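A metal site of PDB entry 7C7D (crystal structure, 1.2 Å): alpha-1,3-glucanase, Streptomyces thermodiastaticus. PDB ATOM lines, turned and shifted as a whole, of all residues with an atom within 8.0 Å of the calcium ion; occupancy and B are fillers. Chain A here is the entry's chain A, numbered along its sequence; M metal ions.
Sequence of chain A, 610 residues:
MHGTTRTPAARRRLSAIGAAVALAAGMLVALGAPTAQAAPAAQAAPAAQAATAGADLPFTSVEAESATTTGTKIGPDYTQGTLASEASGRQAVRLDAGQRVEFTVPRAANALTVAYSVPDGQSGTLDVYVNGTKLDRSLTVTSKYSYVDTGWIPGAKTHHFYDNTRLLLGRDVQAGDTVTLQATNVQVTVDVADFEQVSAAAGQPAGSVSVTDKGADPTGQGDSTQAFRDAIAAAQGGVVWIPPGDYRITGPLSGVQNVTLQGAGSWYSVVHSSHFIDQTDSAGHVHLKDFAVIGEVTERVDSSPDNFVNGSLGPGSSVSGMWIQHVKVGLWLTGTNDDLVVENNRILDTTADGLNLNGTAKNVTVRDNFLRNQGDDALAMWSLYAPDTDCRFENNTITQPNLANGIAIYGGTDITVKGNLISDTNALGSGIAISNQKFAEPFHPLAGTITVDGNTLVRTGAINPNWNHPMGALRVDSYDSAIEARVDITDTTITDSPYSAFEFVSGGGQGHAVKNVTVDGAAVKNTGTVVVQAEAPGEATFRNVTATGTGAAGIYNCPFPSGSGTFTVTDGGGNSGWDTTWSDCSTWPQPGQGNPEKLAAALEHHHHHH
O of Asp 191 sits close to N of Ala 64 (3.0 Å).
N of Asp 191 sits at hydrogen-bond distance from O of Ala 115 (2.8 Å).
OG of Ser 66 is in hydrogen-bond range of O of Glu 63 (2.8 Å).
The side-chain amide nitrogen (NE2) of Gln 91 lies within hydrogen-bond range of the backbone carbonyl oxygen (O) of Gly 89 (3.1 Å).
The calcium ion is bound by the side-chain carboxylate (OD1) of Asp 191 (2.3 Å), the side-chain carboxylate (OE2) of Glu 63 (2.3 Å), the backbone carbonyl oxygen (O) of Gln 91 (2.4 Å), the backbone carbonyl oxygen (O) of Ser 88 (2.4 Å), the side-chain carboxylate (OE1) of Glu 65 (2.5 Å), the side-chain carboxylate (OE2) of Glu 65 (2.5 Å) and the backbone carbonyl oxygen (O) of Asp 191 (2.6 Å).
Of the 23 residues printed, 5 come within 4 Å of the calcium ion.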
ATOM      1  N   VAL A  62      18.657  -1.161  -9.314  1.00  0.00           N
ATOM      2  CA  VAL A  62      19.558  -0.076  -9.680  1.00  0.00           C
ATOM      3  C   VAL A  62      18.712   1.166  -9.911  1.00  0.00           C
ATOM      4  O   VAL A  62      17.813   1.168 -10.766  1.00  0.00           O
ATOM      5  CB  VAL A  62      20.375  -0.412 -10.941  1.00  0.00           C
ATOM      6  CG1 VAL A  62      21.310   0.747 -11.277  1.00  0.00           C
ATOM      7  CG2 VAL A  62      21.153  -1.708 -10.757  1.00  0.00           C
ATOM      8  N   GLU A  63      18.973   2.210  -9.137  1.00  0.00           N
ATOM      9  CA  GLU A  63      18.232   3.457  -9.302  1.00  0.00           C
ATOM     10  C   GLU A  63      18.559   4.065 -10.651  1.00  0.00           C
ATOM     11  O   GLU A  63      19.720   4.109 -11.079  1.00  0.00           O
ATOM     12  CB  GLU A  63      18.591   4.440  -8.188  1.00  0.00           C
ATOM     13  CG  GLU A  63      18.199   3.984  -6.788  1.00  0.00           C
ATOM     14  CD  GLU A  63      16.709   4.018  -6.525  1.00  0.00           C
ATOM     15  OE1 GLU A  63      16.302   3.515  -5.457  1.00  0.00           O
ATOM     16  OE2 GLU A  63      15.942   4.534  -7.367  1.00  0.00           O
ATOM     17  N   ALA A  64      17.534   4.564 -11.346  1.00  0.00           N
ATOM     18  CA  ALA A  64      17.771   5.158 -12.649  1.00  0.00           C
ATOM     19  C   ALA A  64      18.706   6.361 -12.551  1.00  0.00           C
ATOM     20  O   ALA A  64      19.513   6.598 -13.459  1.00  0.00           O
ATOM     21  CB  ALA A  64      16.445   5.561 -13.284  1.00  0.00           C
ATOM     22  N   GLU A  65      18.622   7.109 -11.457  1.00  0.00           N
ATOM     23  CA  GLU A  65      19.456   8.286 -11.269  1.00  0.00           C
ATOM     24  C   GLU A  65      20.923   7.921 -11.058  1.00  0.00           C
ATOM     25  O   GLU A  65      21.770   8.824 -11.110  1.00  0.00           O
ATOM     26  CB  GLU A  65      18.913   9.124 -10.100  1.00  0.00           C
ATOM     27  CG  GLU A  65      18.770   8.356  -8.775  1.00  0.00           C
ATOM     28  CD  GLU A  65      17.405   7.692  -8.554  1.00  0.00           C
ATOM     29  OE1 GLU A  65      16.753   7.304  -9.541  1.00  0.00           O
ATOM     30  OE2 GLU A  65      17.008   7.528  -7.386  1.00  0.00           O
ATOM     31  N   SER A  66      21.238   6.645 -10.832  1.00  0.00           N
ATOM     32  CA  SER A  66      22.617   6.183 -10.739  1.00  0.00           C
ATOM     33  C   SER A  66      23.154   5.642 -12.053  1.00  0.00           C
ATOM     34  O   SER A  66      24.307   5.225 -12.119  1.00  0.00           O
ATOM     35  CB  SER A  66      22.751   5.106  -9.642  1.00  0.00           C
ATOM     36  OG  SER A  66      22.335   3.841 -10.135  1.00  0.00           O
ATOM     37  N   ILE A  74      15.156  14.165 -12.004  1.00  0.00           N
ATOM     38  CA  ILE A  74      14.219  14.908 -11.157  1.00  0.00           C
ATOM     39  C   ILE A  74      14.492  14.538  -9.708  1.00  0.00           C
ATOM     40  O   ILE A  74      14.986  13.447  -9.404  1.00  0.00           O
ATOM     41  CB  ILE A  74      12.734  14.704 -11.517  1.00  0.00           C
ATOM     42  CG1 ILE A  74      12.275  13.267 -11.240  1.00  0.00           C
ATOM     43  CG2 ILE A  74      12.488  15.109 -12.974  1.00  0.00           C
ATOM     44  CD1 ILE A  74      10.766  13.091 -11.309  1.00  0.00           C
ATOM     45  N   ALA A  84       8.542  13.439  -7.872  1.00  0.00           N
ATOM     46  CA  ALA A  84       9.783  12.963  -7.268  1.00  0.00           C
ATOM     47  C   ALA A  84       9.552  12.343  -5.896  1.00  0.00           C
ATOM     48  O   ALA A  84      10.263  11.406  -5.507  1.00  0.00           O
ATOM     49  CB  ALA A  84      10.799  14.099  -7.179  1.00  0.00           C
ATOM     50  N   GLU A  86       7.376  10.359  -4.784  1.00  0.00           N
ATOM     51  CA  GLU A  86       6.991   8.948  -4.829  1.00  0.00           C
ATOM     52  C   GLU A  86       8.039   8.067  -5.481  1.00  0.00           C
ATOM     53  O   GLU A  86       7.837   6.857  -5.583  1.00  0.00           O
ATOM     54  CB  GLU A  86       5.635   8.769  -5.533  1.00  0.00           C
ATOM     55  CG  GLU A  86       4.425   9.170  -4.695  1.00  0.00           C
ATOM     56  CD  GLU A  86       3.121   8.602  -5.225  1.00  0.00           C
ATOM     57  OE1 GLU A  86       3.137   7.979  -6.306  1.00  0.00           O
ATOM     58  OE2 GLU A  86       2.082   8.785  -4.565  1.00  0.00           O
ATOM     59  N   ALA A  87       9.152   8.634  -5.942  1.00  0.00           N
ATOM     60  CA  ALA A  87      10.210   7.829  -6.532  1.00  0.00           C
ATOM     61  C   ALA A  87      11.096   7.223  -5.456  1.00  0.00           C
ATOM     62  O   ALA A  87      11.378   7.848  -4.428  1.00  0.00           O
ATOM     63  CB  ALA A  87      11.068   8.701  -7.448  1.00  0.00           C
ATOM     64  N   SER A  88      11.536   5.982  -5.702  1.00  0.00           N
ATOM     65  CA  SER A  88      12.605   5.395  -4.892  1.00  0.00           C
ATOM     66  C   SER A  88      13.796   6.336  -4.879  1.00  0.00           C
ATOM     67  O   SER A  88      14.243   6.810  -5.927  1.00  0.00           O
ATOM     68  CB  SER A  88      12.983   4.046  -5.511  1.00  0.00           C
ATOM     69  OG  SER A  88      13.869   3.322  -4.675  1.00  0.00           O
ATOM     70  N   GLY A  89      14.327   6.614  -3.685  1.00  0.00           N
ATOM     71  CA  GLY A  89      15.394   7.584  -3.568  1.00  0.00           C
ATOM     72  C   GLY A  89      14.982   9.022  -3.781  1.00  0.00           C
ATOM     73  O   GLY A  89      15.852   9.897  -3.789  1.00  0.00           O
ATOM     74  N   ARG A  90      13.690   9.287  -3.953  1.00  0.00           N
ATOM     75  CA  ARG A  90      13.149  10.622  -4.215  1.00  0.00           C
ATOM     76  C   ARG A  90      13.661  11.209  -5.512  1.00  0.00           C
ATOM     77  O   ARG A  90      13.603  12.430  -5.704  1.00  0.00           O
ATOM     78  CB  ARG A  90      13.365  11.579  -3.042  1.00  0.00           C
ATOM     79  CG  ARG A  90      13.046  10.979  -1.700  1.00  0.00           C
ATOM     80  CD  ARG A  90      11.603  10.451  -1.600  1.00  0.00           C
ATOM     81  NE  ARG A  90      11.418   9.906  -0.264  1.00  0.00           N
ATOM     82  CZ  ARG A  90      10.314   9.996   0.469  1.00  0.00           C
ATOM     83  NH1 ARG A  90       9.215  10.559  -0.025  1.00  0.00           N
ATOM     84  NH2 ARG A  90      10.337   9.517   1.705  1.00  0.00           N
ATOM     85  N   GLN A  91      14.186  10.369  -6.407  1.00  0.00           N
ATOM     86  CA  GLN A  91      14.765  10.819  -7.667  1.00  0.00           C
ATOM     87  C   GLN A  91      14.408   9.834  -8.767  1.00  0.00           C
ATOM     88  O   GLN A  91      14.197   8.645  -8.515  1.00  0.00           O
ATOM     89  CB  GLN A  91      16.290  10.919  -7.579  1.00  0.00           C
ATOM     90  CG  GLN A  91      16.769  11.935  -6.578  1.00  0.00           C
ATOM     91  CD  GLN A  91      18.219  11.719  -6.244  1.00  0.00           C
ATOM     92  OE1 GLN A  91      19.110  12.231  -6.902  1.00  0.00           O
ATOM     93  NE2 GLN A  91      18.468  10.909  -5.210  1.00  0.00           N
ATOM     94  N   ALA A  92      14.341  10.342  -9.987  1.00  0.00           N
ATOM     95  CA  ALA A  92      14.051   9.533 -11.166  1.00  0.00           C
ATOM     96  C   ALA A  92      14.642  10.263 -12.368  1.00  0.00           C
ATOM     97  O   ALA A  92      15.209  11.345 -12.232  1.00  0.00           O
ATOM     98  CB  ALA A  92      12.537   9.311 -11.309  1.00  0.00           C
ATOM     99  N   VAL A  93      14.480   9.663 -13.545  1.00  0.00           N
ATOM    100  CA  VAL A  93      15.029  10.239 -14.776  1.00  0.00           C
ATOM    101  C   VAL A  93      13.911  10.357 -15.793  1.00  0.00           C
ATOM    102  O   VAL A  93      13.313   9.348 -16.183  1.00  0.00           O
ATOM    103  CB  VAL A  93      16.193   9.390 -15.333  1.00  0.00           C
ATOM    104  CG1 VAL A  93      16.696  10.000 -16.626  1.00  0.00           C
ATOM    105  CG2 VAL A  93      17.323   9.289 -14.309  1.00  0.00           C
ATOM    106  N   ALA A 115      10.212   0.332 -12.542  1.00  0.00           N
ATOM    107  CA  ALA A 115       9.235   1.254 -11.953  1.00  0.00           C
ATOM    108  C   ALA A 115       9.333   2.578 -12.700  1.00  0.00           C
ATOM    109  O   ALA A 115      10.426   3.121 -12.875  1.00  0.00           O
ATOM    110  CB  ALA A 115       9.524   1.451 -10.470  1.00  0.00           C
ATOM    111  N   TYR A 162       3.412   6.059 -10.099  1.00  0.00           N
ATOM    112  CA  TYR A 162       4.284   5.091 -10.749  1.00  0.00           C
ATOM    113  C   TYR A 162       3.552   3.770 -10.935  1.00  0.00           C
ATOM    114  O   TYR A 162       2.422   3.576 -10.496  1.00  0.00           O
ATOM    115  CB  TYR A 162       5.586   4.906  -9.927  1.00  0.00           C
ATOM    116  CG  TYR A 162       6.457   6.148  -9.917  1.00  0.00           C
ATOM    117  CD1 TYR A 162       6.211   7.176  -9.007  1.00  0.00           C
ATOM    118  CD2 TYR A 162       7.503   6.306 -10.828  1.00  0.00           C
ATOM    119  CE1 TYR A 162       6.990   8.325  -9.008  1.00  0.00           C
ATOM    120  CE2 TYR A 162       8.280   7.457 -10.843  1.00  0.00           C
ATOM    121  CZ  TYR A 162       8.009   8.458  -9.924  1.00  0.00           C
ATOM    122  OH  TYR A 162       8.776   9.601  -9.945  1.00  0.00           O
ATOM    123  N   VAL A 190      11.662   7.220 -15.467  1.00  0.00           N
ATOM    124  CA  VAL A 190      12.145   5.935 -14.978  1.00  0.00           C
ATOM    125  C   VAL A 190      12.708   6.112 -13.576  1.00  0.00           C
ATOM    126  O   VAL A 190      13.583   6.951 -13.352  1.00  0.00           O
ATOM    127  CB  VAL A 190      13.191   5.349 -15.933  1.00  0.00           C
ATOM    128  CG1 VAL A 190      13.660   3.985 -15.435  1.00  0.00           C
ATOM    129  CG2 VAL A 190      12.617   5.237 -17.349  1.00  0.00           C
ATOM    130  N   ASP A 191      12.211   5.317 -12.636  1.00  0.00           N
ATOM    131  CA  ASP A 191      12.605   5.447 -11.230  1.00  0.00           C
ATOM    132  C   ASP A 191      13.752   4.513 -10.854  1.00  0.00           C
ATOM    133  O   ASP A 191      14.776   4.945 -10.320  1.00  0.00           O
ATOM    134  CB  ASP A 191      11.373   5.156 -10.371  1.00  0.00           C
ATOM    135  CG  ASP A 191      11.650   5.264  -8.887  1.00  0.00           C
ATOM    136  OD1 ASP A 191      12.738   5.763  -8.499  1.00  0.00           O
ATOM    137  OD2 ASP A 191      10.767   4.845  -8.107  1.00  0.00           O
ATOM    138  N   VAL A 192      13.569   3.216 -11.109  1.00  0.00           N
ATOM    139  CA  VAL A 192      14.477   2.172 -10.626  1.00  0.00           C
ATOM    140  C   VAL A 192      14.190   0.932 -11.464  1.00  0.00           C
ATOM    141  O   VAL A 192      13.063   0.731 -11.921  1.00  0.00           O
ATOM    142  CB  VAL A 192      14.278   1.935  -9.104  1.00  0.00           C
ATOM    143  CG1 VAL A 192      12.816   1.641  -8.752  1.00  0.00           C
ATOM    144  CG2 VAL A 192      15.207   0.823  -8.586  1.00  0.00           C
ATOM    145  N   ALA A 193      15.221   0.131 -11.699  1.00  0.00           N
ATOM    146  CA  ALA A 193      15.085  -1.115 -12.435  1.00  0.00           C
ATOM    147  C   ALA A 193      15.601  -2.275 -11.596  1.00  0.00           C
ATOM    148  O   ALA A 193      16.638  -2.140 -10.926  1.00  0.00           O
ATOM    149  CB  ALA A 193      15.846  -1.057 -13.761  1.00  0.00           C
ATOM    150  N   ASP A 424      11.519   5.190   2.091  1.00  0.00           N
ATOM    151  CA  ASP A 424      10.800   6.193   1.315  1.00  0.00           C
ATOM    152  C   ASP A 424       9.295   6.159   1.574  1.00  0.00           C
ATOM    153  O   ASP A 424       8.494   5.762   0.727  1.00  0.00           O
ATOM    154  CB  ASP A 424      11.084   6.032  -0.183  1.00  0.00           C
ATOM    155  CG  ASP A 424      12.510   6.406  -0.544  1.00  0.00           C
ATOM    156  OD1 ASP A 424      12.945   7.498  -0.133  1.00  0.00           O
ATOM    157  OD2 ASP A 424      13.182   5.605  -1.233  1.00  0.00           O
ATOM    158  N   ARG A 459      15.002   7.117   4.854  1.00  0.00           N
ATOM    159  CA  ARG A 459      14.193   8.208   4.290  1.00  0.00           C
ATOM    160  C   ARG A 459      12.712   8.021   4.619  1.00  0.00           C
ATOM    161  O   ARG A 459      11.844   8.151   3.749  1.00  0.00           O
ATOM    162  CB  ARG A 459      14.427   8.385   2.786  1.00  0.00           C
ATOM    163  CG  ARG A 459      15.872   8.785   2.425  1.00  0.00           C
ATOM    164  CD  ARG A 459      16.064   8.952   0.903  1.00  0.00           C
ATOM    165  NE  ARG A 459      15.697   7.720   0.206  1.00  0.00           N
ATOM    166  CZ  ARG A 459      16.505   6.687   0.001  1.00  0.00           C
ATOM    167  NH1 ARG A 459      17.783   6.760   0.370  1.00  0.00           N
ATOM    168  NH2 ARG A 459      16.059   5.575  -0.554  1.00  0.00           N
HETATM  169 CA    CA M   1      14.898   6.405  -8.189  1.00  0.00          CA
